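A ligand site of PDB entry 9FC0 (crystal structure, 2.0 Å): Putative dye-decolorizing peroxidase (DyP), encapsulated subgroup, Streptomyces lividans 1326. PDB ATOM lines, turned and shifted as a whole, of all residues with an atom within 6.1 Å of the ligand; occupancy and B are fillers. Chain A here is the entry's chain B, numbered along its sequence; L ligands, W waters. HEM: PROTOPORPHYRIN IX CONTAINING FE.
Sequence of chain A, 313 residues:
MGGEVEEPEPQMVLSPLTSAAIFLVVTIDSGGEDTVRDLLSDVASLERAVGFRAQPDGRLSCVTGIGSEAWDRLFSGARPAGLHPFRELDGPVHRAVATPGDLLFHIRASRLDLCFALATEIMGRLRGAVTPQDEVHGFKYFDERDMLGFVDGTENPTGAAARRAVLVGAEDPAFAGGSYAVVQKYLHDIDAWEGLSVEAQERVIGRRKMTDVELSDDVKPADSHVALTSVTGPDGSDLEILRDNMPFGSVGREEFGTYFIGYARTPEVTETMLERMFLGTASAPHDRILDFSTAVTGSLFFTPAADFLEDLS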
ATOM      1  N   ASP A 146       5.074  17.778  19.303  1.00  0.00           N
ATOM      2  CA  ASP A 146       4.901  17.760  17.867  1.00  0.00           C
ATOM      3  C   ASP A 146       3.943  18.880  17.445  1.00  0.00           C
ATOM      4  O   ASP A 146       3.484  19.677  18.282  1.00  0.00           O
ATOM      5  CB  ASP A 146       4.544  16.360  17.403  1.00  0.00           C
ATOM      6  CG  ASP A 146       3.231  15.824  17.949  1.00  0.00           C
ATOM      7  OD1 ASP A 146       2.384  16.638  18.287  1.00  0.00           O
ATOM      8  OD2 ASP A 146       3.123  14.568  18.050  1.00  0.00           O
ATOM      9  N   LEU A 148       0.836  18.709  16.736  1.00  0.00           N
ATOM     10  CA  LEU A 148      -0.482  18.586  17.395  1.00  0.00           C
ATOM     11  C   LEU A 148      -0.450  19.086  18.850  1.00  0.00           C
ATOM     12  O   LEU A 148      -1.503  19.146  19.500  1.00  0.00           O
ATOM     13  CB  LEU A 148      -0.935  17.127  17.309  1.00  0.00           C
ATOM     14  CG  LEU A 148      -1.121  16.589  15.875  1.00  0.00           C
ATOM     15  CD1 LEU A 148      -1.719  15.211  15.823  1.00  0.00           C
ATOM     16  CD2 LEU A 148      -1.966  17.529  15.019  1.00  0.00           C
ATOM     17  N   PHE A 150       1.231  17.610  21.381  1.00  0.00           N
ATOM     18  CA  PHE A 150       1.466  16.510  22.302  1.00  0.00           C
ATOM     19  C   PHE A 150       2.958  16.158  22.348  1.00  0.00           C
ATOM     20  O   PHE A 150       3.664  16.268  21.338  1.00  0.00           O
ATOM     21  CB  PHE A 150       0.666  15.260  21.899  1.00  0.00           C
ATOM     22  CG  PHE A 150      -0.790  15.330  22.290  1.00  0.00           C
ATOM     23  CD1 PHE A 150      -1.643  16.257  21.711  1.00  0.00           C
ATOM     24  CD2 PHE A 150      -1.264  14.547  23.322  1.00  0.00           C
ATOM     25  CE1 PHE A 150      -2.945  16.382  22.160  1.00  0.00           C
ATOM     26  CE2 PHE A 150      -2.561  14.676  23.779  1.00  0.00           C
ATOM     27  CZ  PHE A 150      -3.400  15.588  23.187  1.00  0.00           C
ATOM     28  N   VAL A 151       3.412  15.733  23.535  1.00  0.00           N
ATOM     29  CA  VAL A 151       4.751  15.175  23.676  1.00  0.00           C
ATOM     30  C   VAL A 151       4.845  13.920  22.804  1.00  0.00           C
ATOM     31  O   VAL A 151       3.960  13.081  22.804  1.00  0.00           O
ATOM     32  CB  VAL A 151       5.084  14.865  25.143  1.00  0.00           C
ATOM     33  CG1 VAL A 151       6.517  14.286  25.238  1.00  0.00           C
ATOM     34  CG2 VAL A 151       4.883  16.116  26.029  1.00  0.00           C
ATOM     35  N   ASP A 152       5.950  13.795  22.080  1.00  0.00           N
ATOM     36  CA  ASP A 152       6.108  12.813  21.033  1.00  0.00           C
ATOM     37  C   ASP A 152       7.483  12.145  21.182  1.00  0.00           C
ATOM     38  O   ASP A 152       8.513  12.808  21.032  1.00  0.00           O
ATOM     39  CB  ASP A 152       5.954  13.524  19.689  1.00  0.00           C
ATOM     40  CG  ASP A 152       5.759  12.620  18.470  1.00  0.00           C
ATOM     41  OD1 ASP A 152       6.374  11.603  18.438  1.00  0.00           O
ATOM     42  OD2 ASP A 152       4.987  13.037  17.542  1.00  0.00           O
ATOM     43  N   GLY A 153       7.503  10.833  21.462  1.00  0.00           N
ATOM     44  CA  GLY A 153       8.705  10.056  21.707  1.00  0.00           C
ATOM     45  C   GLY A 153       8.677   9.247  23.031  1.00  0.00           C
ATOM     46  O   GLY A 153       9.508   8.370  23.281  1.00  0.00           O
ATOM     47  N   THR A 154       7.707   9.555  23.900  1.00  0.00           N
ATOM     48  CA  THR A 154       7.726   9.134  25.294  1.00  0.00           C
ATOM     49  C   THR A 154       7.932   7.627  25.435  1.00  0.00           C
ATOM     50  O   THR A 154       8.727   7.206  26.237  1.00  0.00           O
ATOM     51  CB  THR A 154       6.424   9.546  25.966  1.00  0.00           C
ATOM     52  OG1 THR A 154       6.236  10.947  25.703  1.00  0.00           O
ATOM     53  CG2 THR A 154       6.399   9.211  27.457  1.00  0.00           C
ATOM     54  N   GLU A 155       7.169   6.796  24.723  1.00  0.00           N
ATOM     55  CA  GLU A 155       7.201   5.352  24.935  1.00  0.00           C
ATOM     56  C   GLU A 155       8.218   4.653  24.045  1.00  0.00           C
ATOM     57  O   GLU A 155       8.193   3.422  23.944  1.00  0.00           O
ATOM     58  CB  GLU A 155       5.800   4.745  24.797  1.00  0.00           C
ATOM     59  CG  GLU A 155       4.891   5.008  26.008  1.00  0.00           C
ATOM     60  CD  GLU A 155       5.462   4.440  27.297  1.00  0.00           C
ATOM     61  OE1 GLU A 155       5.587   3.226  27.301  1.00  0.00           O
ATOM     62  OE2 GLU A 155       5.786   5.187  28.263  1.00  0.00           O
ATOM     63  N   ASN A 156       9.111   5.419  23.366  1.00  0.00           N
ATOM     64  CA  ASN A 156      10.172   4.749  22.626  1.00  0.00           C
ATOM     65  C   ASN A 156      10.969   3.854  23.577  1.00  0.00           C
ATOM     66  O   ASN A 156      11.283   4.257  24.723  1.00  0.00           O
ATOM     67  CB  ASN A 156      11.181   5.705  22.011  1.00  0.00           C
ATOM     68  CG  ASN A 156      10.816   6.195  20.625  1.00  0.00           C
ATOM     69  OD1 ASN A 156      10.207   5.497  19.830  1.00  0.00           O
ATOM     70  ND2 ASN A 156      11.221   7.420  20.312  1.00  0.00           N
ATOM     71  N   GLN A 184       6.832   8.231   6.256  1.00  0.00           N
ATOM     72  CA  GLN A 184       5.620   8.834   5.712  1.00  0.00           C
ATOM     73  C   GLN A 184       5.581  10.309   6.084  1.00  0.00           C
ATOM     74  O   GLN A 184       5.671  10.685   7.250  1.00  0.00           O
ATOM     75  CB  GLN A 184       4.331   8.217   6.273  1.00  0.00           C
ATOM     76  CG  GLN A 184       4.163   6.708   6.029  1.00  0.00           C
ATOM     77  CD  GLN A 184       2.899   6.227   6.684  1.00  0.00           C
ATOM     78  OE1 GLN A 184       2.779   6.216   7.916  1.00  0.00           O
ATOM     79  NE2 GLN A 184       1.905   5.941   5.874  1.00  0.00           N
ATOM     80  N   TYR A 186       3.281  13.425   6.639  1.00  0.00           N
ATOM     81  CA  TYR A 186       1.906  13.724   6.955  1.00  0.00           C
ATOM     82  C   TYR A 186       1.701  15.227   6.943  1.00  0.00           C
ATOM     83  O   TYR A 186       2.522  15.957   7.531  1.00  0.00           O
ATOM     84  CB  TYR A 186       1.506  13.166   8.326  1.00  0.00           C
ATOM     85  CG  TYR A 186       1.270  11.669   8.459  1.00  0.00           C
ATOM     86  CD1 TYR A 186       2.324  10.781   8.695  1.00  0.00           C
ATOM     87  CD2 TYR A 186       0.012  11.122   8.192  1.00  0.00           C
ATOM     88  CE1 TYR A 186       2.111   9.409   8.764  1.00  0.00           C
ATOM     89  CE2 TYR A 186      -0.210   9.754   8.238  1.00  0.00           C
ATOM     90  CZ  TYR A 186       0.851   8.886   8.511  1.00  0.00           C
ATOM     91  OH  TYR A 186       0.615   7.549   8.614  1.00  0.00           O
ATOM     92  N   HIS A 188      -1.187  18.009   8.309  1.00  0.00           N
ATOM     93  CA  HIS A 188      -2.289  18.100   9.239  1.00  0.00           C
ATOM     94  C   HIS A 188      -3.276  19.202   8.855  1.00  0.00           C
ATOM     95  O   HIS A 188      -2.926  20.206   8.242  1.00  0.00           O
ATOM     96  CB  HIS A 188      -1.763  18.377  10.651  1.00  0.00           C
ATOM     97  CG  HIS A 188      -0.891  17.300  11.192  1.00  0.00           C
ATOM     98  ND1 HIS A 188      -1.390  16.054  11.471  1.00  0.00           N
ATOM     99  CD2 HIS A 188       0.419  17.303  11.512  1.00  0.00           C
ATOM    100  CE1 HIS A 188      -0.357  15.311  11.887  1.00  0.00           C
ATOM    101  NE2 HIS A 188       0.720  16.075  11.988  1.00  0.00           N
ATOM    102  N   ILE A 205      -5.502  10.847  20.929  1.00  0.00           N
ATOM    103  CA  ILE A 205      -4.123  10.355  21.063  1.00  0.00           C
ATOM    104  C   ILE A 205      -4.079   9.179  22.035  1.00  0.00           C
ATOM    105  O   ILE A 205      -3.455   8.178  21.747  1.00  0.00           O
ATOM    106  CB  ILE A 205      -3.225  11.532  21.533  1.00  0.00           C
ATOM    107  CG1 ILE A 205      -3.216  12.710  20.553  1.00  0.00           C
ATOM    108  CG2 ILE A 205      -1.801  11.035  21.858  1.00  0.00           C
ATOM    109  CD1 ILE A 205      -2.684  12.372  19.213  1.00  0.00           C
ATOM    110  N   ARG A 207      -3.455   9.961  25.595  1.00  0.00           N
ATOM    111  CA  ARG A 207      -2.604  10.469  26.672  1.00  0.00           C
ATOM    112  C   ARG A 207      -3.088  11.852  27.026  1.00  0.00           C
ATOM    113  O   ARG A 207      -3.652  12.513  26.155  1.00  0.00           O
ATOM    114  CB  ARG A 207      -1.121  10.516  26.231  1.00  0.00           C
ATOM    115  CG  ARG A 207      -0.555   9.232  25.677  1.00  0.00           C
ATOM    116  CD  ARG A 207       0.943   9.308  25.339  1.00  0.00           C
ATOM    117  NE  ARG A 207       1.800   9.355  26.529  1.00  0.00           N
ATOM    118  CZ  ARG A 207       2.188   8.266  27.214  1.00  0.00           C
ATOM    119  NH1 ARG A 207       2.618   8.399  28.451  1.00  0.00           N
ATOM    120  NH2 ARG A 207       2.090   7.041  26.696  1.00  0.00           N
ATOM    121  N   ASP A 212       1.227  14.318  29.881  1.00  0.00           N
ATOM    122  CA  ASP A 212       1.738  13.203  29.097  1.00  0.00           C
ATOM    123  C   ASP A 212       1.590  11.885  29.861  1.00  0.00           C
ATOM    124  O   ASP A 212       2.230  10.918  29.534  1.00  0.00           O
ATOM    125  CB  ASP A 212       3.181  13.395  28.670  1.00  0.00           C
ATOM    126  CG  ASP A 212       3.683  12.464  27.570  1.00  0.00           C
ATOM    127  OD1 ASP A 212       2.875  11.959  26.834  1.00  0.00           O
ATOM    128  OD2 ASP A 212       4.885  12.286  27.449  1.00  0.00           O
ATOM    129  N   GLU A 214      -0.523   8.574  30.303  1.00  0.00           N
ATOM    130  CA  GLU A 214      -1.393   7.721  29.527  1.00  0.00           C
ATOM    131  C   GLU A 214      -2.769   7.606  30.179  1.00  0.00           C
ATOM    132  O   GLU A 214      -2.856   7.542  31.393  1.00  0.00           O
ATOM    133  CB  GLU A 214      -0.710   6.353  29.427  1.00  0.00           C
ATOM    134  CG  GLU A 214      -1.452   5.376  28.535  1.00  0.00           C
ATOM    135  CD  GLU A 214      -0.680   4.100  28.271  1.00  0.00           C
ATOM    136  OE1 GLU A 214       0.502   4.025  28.643  1.00  0.00           O
ATOM    137  OE2 GLU A 214      -1.262   3.200  27.702  1.00  0.00           O
ATOM    138  N   HIS A 225      -4.895   6.637  19.069  1.00  0.00           N
ATOM    139  CA  HIS A 225      -3.598   6.337  18.457  1.00  0.00           C
ATOM    140  C   HIS A 225      -2.815   5.323  19.274  1.00  0.00           C
ATOM    141  O   HIS A 225      -2.247   4.377  18.738  1.00  0.00           O
ATOM    142  CB  HIS A 225      -2.790   7.642  18.256  1.00  0.00           C
ATOM    143  CG  HIS A 225      -1.556   7.472  17.490  1.00  0.00           C
ATOM    144  ND1 HIS A 225      -1.516   6.840  16.261  1.00  0.00           N
ATOM    145  CD2 HIS A 225      -0.290   7.826  17.773  1.00  0.00           C
ATOM    146  CE1 HIS A 225      -0.247   6.803  15.826  1.00  0.00           C
ATOM    147  NE2 HIS A 225       0.508   7.404  16.721  1.00  0.00           N
ATOM    148  N   VAL A 226      -2.771   5.550  20.592  1.00  0.00           N
ATOM    149  CA  VAL A 226      -1.970   4.702  21.467  1.00  0.00           C
ATOM    150  C   VAL A 226      -2.547   3.284  21.523  1.00  0.00           C
ATOM    151  O   VAL A 226      -1.762   2.325  21.600  1.00  0.00           O
ATOM    152  CB  VAL A 226      -1.828   5.305  22.868  1.00  0.00           C
ATOM    153  CG1 VAL A 226      -1.383   4.267  23.912  1.00  0.00           C
ATOM    154  CG2 VAL A 226      -0.868   6.473  22.861  1.00  0.00           C
ATOM    155  N   THR A 229      -1.668   1.419  18.129  1.00  0.00           N
ATOM    156  CA  THR A 229      -0.267   1.163  17.789  1.00  0.00           C
ATOM    157  C   THR A 229       0.405   0.346  18.890  1.00  0.00           C
ATOM    158  O   THR A 229       1.615   0.193  18.878  1.00  0.00           O
ATOM    159  CB  THR A 229       0.467   2.481  17.486  1.00  0.00           C
ATOM    160  OG1 THR A 229       0.416   3.407  18.573  1.00  0.00           O
ATOM    161  CG2 THR A 229      -0.097   3.146  16.258  1.00  0.00           C
ATOM    162  N   SER A 230      -0.369  -0.101  19.895  1.00  0.00           N
ATOM    163  CA  SER A 230       0.062  -1.076  20.903  1.00  0.00           C
ATOM    164  C   SER A 230      -0.221  -2.486  20.398  1.00  0.00           C
ATOM    165  O   SER A 230      -1.375  -2.837  20.236  1.00  0.00           O
ATOM    166  CB  SER A 230      -0.628  -0.856  22.219  1.00  0.00           C
ATOM    167  OG  SER A 230      -0.279   0.417  22.728  1.00  0.00           O
ATOM    168  N   ILE A 241       8.740  -0.379  18.194  1.00  0.00           N
ATOM    169  CA  ILE A 241       9.547   0.305  17.216  1.00  0.00           C
ATOM    170  C   ILE A 241      10.173   1.552  17.839  1.00  0.00           C
ATOM    171  O   ILE A 241       9.764   2.000  18.885  1.00  0.00           O
ATOM    172  CB  ILE A 241       8.731   0.645  15.959  1.00  0.00           C
ATOM    173  CG1 ILE A 241       7.699   1.727  16.196  1.00  0.00           C
ATOM    174  CG2 ILE A 241       8.114  -0.607  15.358  1.00  0.00           C
ATOM    175  CD1 ILE A 241       7.112   2.243  14.853  1.00  0.00           C
ATOM    176  N   ARG A 243      10.897   5.518  16.995  1.00  0.00           N
ATOM    177  CA  ARG A 243      10.407   6.609  16.155  1.00  0.00           C
ATOM    178  C   ARG A 243      11.192   7.867  16.449  1.00  0.00           C
ATOM    179  O   ARG A 243      11.694   8.046  17.569  1.00  0.00           O
ATOM    180  CB  ARG A 243       8.936   6.926  16.481  1.00  0.00           C
ATOM    181  CG  ARG A 243       7.971   5.796  16.168  1.00  0.00           C
ATOM    182  CD  ARG A 243       6.633   6.007  16.836  1.00  0.00           C
ATOM    183  NE  ARG A 243       6.702   5.826  18.294  1.00  0.00           N
ATOM    184  CZ  ARG A 243       6.457   6.760  19.214  1.00  0.00           C
ATOM    185  NH1 ARG A 243       5.998   7.944  18.880  1.00  0.00           N
ATOM    186  NH2 ARG A 243       6.702   6.511  20.500  1.00  0.00           N
ATOM    187  N   ASN A 245       9.910  11.199  15.017  1.00  0.00           N
ATOM    188  CA  ASN A 245       9.027  12.069  14.282  1.00  0.00           C
ATOM    189  C   ASN A 245       9.441  13.542  14.435  1.00  0.00           C
ATOM    190  O   ASN A 245       9.776  14.032  15.536  1.00  0.00           O
ATOM    191  CB  ASN A 245       7.587  11.935  14.804  1.00  0.00           C
ATOM    192  CG  ASN A 245       6.980  10.568  14.636  1.00  0.00           C
ATOM    193  OD1 ASN A 245       7.527   9.709  13.929  1.00  0.00           O
ATOM    194  ND2 ASN A 245       5.970  10.322  15.453  1.00  0.00           N
ATOM    195  N   THR A 258       3.881  16.501  10.151  1.00  0.00           N
ATOM    196  CA  THR A 258       4.719  15.584  10.886  1.00  0.00           C
ATOM    197  C   THR A 258       5.414  14.667   9.904  1.00  0.00           C
ATOM    198  O   THR A 258       4.753  13.983   9.146  1.00  0.00           O
ATOM    199  CB  THR A 258       3.925  14.725  11.881  1.00  0.00           C
ATOM    200  OG1 THR A 258       3.268  15.580  12.809  1.00  0.00           O
ATOM    201  CG2 THR A 258       4.801  13.791  12.692  1.00  0.00           C
ATOM    202  N   PHE A 260       7.051  11.301   9.783  1.00  0.00           N
ATOM    203  CA  PHE A 260       7.110  10.046  10.519  1.00  0.00           C
ATOM    204  C   PHE A 260       8.273   9.230   9.994  1.00  0.00           C
ATOM    205  O   PHE A 260       8.411   9.032   8.792  1.00  0.00           O
ATOM    206  CB  PHE A 260       5.831   9.203  10.325  1.00  0.00           C
ATOM    207  CG  PHE A 260       5.954   7.812  10.901  1.00  0.00           C
ATOM    208  CD1 PHE A 260       5.804   7.575  12.264  1.00  0.00           C
ATOM    209  CD2 PHE A 260       6.248   6.720  10.082  1.00  0.00           C
ATOM    210  CE1 PHE A 260       5.968   6.297  12.785  1.00  0.00           C
ATOM    211  CE2 PHE A 260       6.448   5.483  10.623  1.00  0.00           C
ATOM    212  CZ  PHE A 260       6.273   5.263  11.955  1.00  0.00           C
ATOM    213  N   THR A 270       6.140  -2.810  11.975  1.00  0.00           N
ATOM    214  CA  THR A 270       5.671  -1.517  11.515  1.00  0.00           C
ATOM    215  C   THR A 270       4.435  -1.664  10.614  1.00  0.00           C
ATOM    216  O   THR A 270       3.486  -0.878  10.710  1.00  0.00           O
ATOM    217  CB  THR A 270       6.786  -0.752  10.793  1.00  0.00           C
ATOM    218  OG1 THR A 270       7.992  -0.862  11.524  1.00  0.00           O
ATOM    219  CG2 THR A 270       6.450   0.707  10.627  1.00  0.00           C
ATOM    220  N   MET A 273       1.230  -2.315  12.566  1.00  0.00           N
ATOM    221  CA  MET A 273       0.731  -1.066  13.149  1.00  0.00           C
ATOM    222  C   MET A 273       0.014  -0.231  12.078  1.00  0.00           C
ATOM    223  O   MET A 273      -1.050   0.334  12.380  1.00  0.00           O
ATOM    224  CB  MET A 273       1.857  -0.223  13.752  1.00  0.00           C
ATOM    225  CG  MET A 273       2.463  -0.832  14.966  1.00  0.00           C
ATOM    226  SD  MET A 273       3.930   0.013  15.542  1.00  0.00           S
ATOM    227  CE  MET A 273       4.205  -0.832  17.097  1.00  0.00           C
ATOM    228  N   LEU A 274       0.579  -0.127  10.864  1.00  0.00           N
ATOM    229  CA  LEU A 274      -0.047   0.601   9.779  1.00  0.00           C
ATOM    230  C   LEU A 274      -1.411   0.006   9.397  1.00  0.00           C
ATOM    231  O   LEU A 274      -2.353   0.738   9.135  1.00  0.00           O
ATOM    232  CB  LEU A 274       0.903   0.641   8.570  1.00  0.00           C
ATOM    233  CG  LEU A 274       2.051   1.659   8.703  1.00  0.00           C
ATOM    234  CD1 LEU A 274       3.121   1.485   7.631  1.00  0.00           C
ATOM    235  CD2 LEU A 274       1.542   3.085   8.671  1.00  0.00           C
ATOM    236  N   MET A 277      -3.971   1.000  11.937  1.00  0.00           N
ATOM    237  CA  MET A 277      -4.332   2.408  11.837  1.00  0.00           C
ATOM    238  C   MET A 277      -5.284   2.677  10.659  1.00  0.00           C
ATOM    239  O   MET A 277      -6.229   3.457  10.805  1.00  0.00           O
ATOM    240  CB  MET A 277      -3.051   3.267  11.654  1.00  0.00           C
ATOM    241  CG  MET A 277      -2.194   3.381  12.925  1.00  0.00           C
ATOM    242  SD  MET A 277      -0.649   4.286  12.536  1.00  0.00           S
ATOM    243  CE  MET A 277      -1.311   5.897  12.083  1.00  0.00           C
ATOM    244  N   PHE A 278      -4.948   2.153   9.466  1.00  0.00           N
ATOM    245  CA  PHE A 278      -5.618   2.464   8.212  1.00  0.00           C
ATOM    246  C   PHE A 278      -6.844   1.567   7.937  1.00  0.00           C
ATOM    247  O   PHE A 278      -7.816   2.059   7.356  1.00  0.00           O
ATOM    248  CB  PHE A 278      -4.623   2.455   7.064  1.00  0.00           C
ATOM    249  CG  PHE A 278      -3.745   3.681   6.962  1.00  0.00           C
ATOM    250  CD1 PHE A 278      -2.583   3.790   7.723  1.00  0.00           C
ATOM    251  CD2 PHE A 278      -4.143   4.772   6.219  1.00  0.00           C
ATOM    252  CE1 PHE A 278      -1.845   4.972   7.766  1.00  0.00           C
ATOM    253  CE2 PHE A 278      -3.377   5.935   6.229  1.00  0.00           C
ATOM    254  CZ  PHE A 278      -2.205   6.012   6.962  1.00  0.00           C
ATOM    255  N   ILE A 289      -6.302   9.643  14.677  1.00  0.00           N
ATOM    256  CA  ILE A 289      -5.295  10.636  14.299  1.00  0.00           C
ATOM    257  C   ILE A 289      -5.372  10.883  12.799  1.00  0.00           C
ATOM    258  O   ILE A 289      -5.021  11.997  12.333  1.00  0.00           O
ATOM    259  CB  ILE A 289      -3.878  10.232  14.798  1.00  0.00           C
ATOM    260  CG1 ILE A 289      -3.030  11.452  15.149  1.00  0.00           C
ATOM    261  CG2 ILE A 289      -3.159   9.319  13.812  1.00  0.00           C
ATOM    262  CD1 ILE A 289      -1.649  11.126  15.731  1.00  0.00           C
ATOM    263  N   SER A 293      -4.880  14.068   9.759  1.00  0.00           N
ATOM    264  CA  SER A 293      -3.552  13.807   9.224  1.00  0.00           C
ATOM    265  C   SER A 293      -3.649  13.007   7.907  1.00  0.00           C
ATOM    266  O   SER A 293      -4.138  11.887   7.913  1.00  0.00           O
ATOM    267  CB  SER A 293      -2.664  13.019  10.219  1.00  0.00           C
ATOM    268  OG  SER A 293      -2.705  13.509  11.571  1.00  0.00           O
HETATM  269  CHA HEM L   1       2.832   7.125  20.068  1.00  0.00           C
HETATM  270  CHB HEM L   1       2.130  11.158  17.429  1.00  0.00           C
HETATM  271  CHC HEM L   1       2.197   8.504  13.382  1.00  0.00           C
HETATM  272  CHD HEM L   1       3.356   4.646  16.015  1.00  0.00           C
HETATM  273  C1A HEM L   1       2.574   8.442  19.686  1.00  0.00           C
HETATM  274  C2A HEM L   1       2.340   9.495  20.590  1.00  0.00           C
HETATM  275  C3A HEM L   1       2.182  10.638  19.830  1.00  0.00           C
HETATM  276  C4A HEM L   1       2.287  10.296  18.505  1.00  0.00           C
HETATM  277  CMA HEM L   1       1.909  12.059  20.305  1.00  0.00           C
HETATM  278  CAA HEM L   1       2.290   9.403  22.100  1.00  0.00           C
HETATM  279  CBA HEM L   1       3.591   9.641  22.890  1.00  0.00           C
HETATM  280  CGA HEM L   1       4.675   8.682  22.421  1.00  0.00           C
HETATM  281  O1A HEM L   1       5.445   9.016  21.462  1.00  0.00           O
HETATM  282  O2A HEM L   1       4.817   7.535  22.901  1.00  0.00           O
HETATM  283  C1B HEM L   1       2.114  10.740  16.100  1.00  0.00           C
HETATM  284  C2B HEM L   1       1.809  11.638  14.942  1.00  0.00           C
HETATM  285  C3B HEM L   1       1.862  10.912  13.854  1.00  0.00           C
HETATM  286  C4B HEM L   1       2.103   9.536  14.289  1.00  0.00           C
HETATM  287  CMB HEM L   1       1.632  13.157  15.070  1.00  0.00           C
HETATM  288  CAB HEM L   1       1.634  11.128  12.448  1.00  0.00           C
HETATM  289  CBB HEM L   1       0.760  11.952  12.048  1.00  0.00           C
HETATM  290  C1C HEM L   1       2.485   7.209  13.747  1.00  0.00           C
HETATM  291  C2C HEM L   1       2.599   6.094  12.883  1.00  0.00           C
HETATM  292  C3C HEM L   1       2.964   4.966  13.613  1.00  0.00           C
HETATM  293  C4C HEM L   1       3.011   5.460  14.998  1.00  0.00           C
HETATM  294  CMC HEM L   1       2.496   6.087  11.399  1.00  0.00           C
HETATM  295  CAC HEM L   1       3.235   3.510  13.207  1.00  0.00           C
HETATM  296  CBC HEM L   1       3.282   2.996  11.990  1.00  0.00           C
HETATM  297  C1D HEM L   1       3.321   5.038  17.336  1.00  0.00           C
HETATM  298  C2D HEM L   1       3.643   4.126  18.453  1.00  0.00           C
HETATM  299  C3D HEM L   1       3.474   4.779  19.545  1.00  0.00           C
HETATM  300  C4D HEM L   1       3.044   6.141  19.142  1.00  0.00           C
HETATM  301  CMD HEM L   1       4.032   2.682  18.427  1.00  0.00           C
HETATM  302  CAD HEM L   1       3.650   4.236  20.919  1.00  0.00           C
HETATM  303  CBD HEM L   1       2.351   3.570  21.434  1.00  0.00           C
HETATM  304  CGD HEM L   1       2.622   2.962  22.847  1.00  0.00           C
HETATM  305  O1D HEM L   1       2.360   3.619  23.891  1.00  0.00           O
HETATM  306  O2D HEM L   1       3.215   1.876  22.938  1.00  0.00           O
HETATM  307  NA  HEM L   1       2.503   8.944  18.409  1.00  0.00           N
HETATM  308  NB  HEM L   1       2.175   9.513  15.653  1.00  0.00           N
HETATM  309  NC  HEM L   1       2.667   6.790  15.055  1.00  0.00           N
HETATM  310  ND  HEM L   1       2.988   6.263  17.769  1.00  0.00           N
HETATM  311 FE   HEM L   1       2.621   7.845  16.747  1.00  0.00          FE
HETATM  312  O   HOH W   1       2.332   6.439  23.961  1.00  0.00           O
HETATM  313  O   HOH W   2       3.820   0.406  20.956  1.00  0.00           O
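N of Thr 154 sits at hydrogen-bond distance from O1A of the ligand (3.4 Å). FE of the ligand is bound by NE2 of His 225 (2.2 Å). N of Glu 155 sits at hydrogen-bond distance from O2A of the ligand (3.1 Å). N of Gly 153 lies within hydrogen-bond range of O1A of the ligand. An oxygen (O1A) of the ligand lies within salt-bridge range of the guanidinium group (NH1) of Arg 243.
The side-chain carboxylate (OD2) of Asp 146 sits close to the side-chain carboxylate (OD2) of Asp 152. The side-chain carboxylate (OD1) of Asp 212 is in salt-bridge range of the guanidinium group (NE) of Arg 207 (2.8 Å). The side-chain amide oxygen (OE1) of Gln 184 lies within hydrogen-bond range of the side-chain hydroxyl (OH) of Tyr 186, at 2.6 Å. The backbone NH of Phe 260 lies within hydrogen-bond range of the backbone carbonyl oxygen of Gln 184 (2.9 Å). OD2 of Asp 212 lies within hydrogen-bond range of OG1 of Thr 154 (2.6 Å). N of His 225 sits at hydrogen-bond distance from O of Ile 205 (3.4 Å). The backbone NH of Leu 148 is in hydrogen-bond range of the side-chain carboxylate of Asp 146, at 3.0 Å. The side-chain amide nitrogen (ND2) of Asn 245 lies within hydrogen-bond range of the side-chain carboxylate (OD1) of Asp 152, at 3.3 Å.
Asp 146 touches the ligand (OD2 to CMA, 3.6 Å). CB of Phe 150 touches CMA of the ligand, at 3.8 Å. Val 151 touches the ligand. Asp 152 touches the ligand (OD2 to CHB, 3.4 Å). OE1 of Gln 184 touches CMC of the ligand (3.5 Å). Tyr 186 touches the ligand. His 188 touches the ligand (CE1 to CBB, 3.5 Å). Arg 207 touches the ligand. Val 226 touches the ligand (CG1 to O1D, 3.8 Å). Thr 229 touches the ligand. Ser 230 touches the ligand. Asn 245 touches the ligand. Thr 258 touches the ligand. CE1 of Phe 260 touches C2C of the ligand, 3.4 Å away. CE of Met 273 touches CMD of the ligand, at 3.8 Å. CD2 of Leu 274 touches CBC of the ligand (3.7 Å). Met 277 touches the ligand. CD1 of Ile 289 touches C2B of the ligand, at 3.6 Å. Ser 293 touches the ligand. Hydrophobic or aromatic side chains within 4 Å of the ligand: Phe 150, Tyr 186, His 188, His 225, Val 226, Phe 260, Met 273, Leu 274, Met 277 and Ile 289. 24 residues have an atom within 4 Å of the ligand: Asp 146, Phe 150, Val 151, Asp 152, Gly 153, Thr 154, Glu 155, Gln 184, Tyr 186, His 188, Arg 207, His 225, Val 226, Thr 229, Ser 230, Arg 243, Asn 245, Thr 258, Phe 260, Met 273, Leu 274, Met 277, Ile 289 and Ser 293. Along chain A the residues within 4 Å of the ligand span positions 146 to 293. The nearest printed residue that does not touch the ligand is Leu 148 (4.002 Å).
Water W2 lies within hydrogen-bond range of O2D of the ligand and O of Thr 229. Water W1 bridges the guanidinium group of Arg 207 (2.8 Å) and an oxygen (O1D) of the ligand (2.8 Å).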
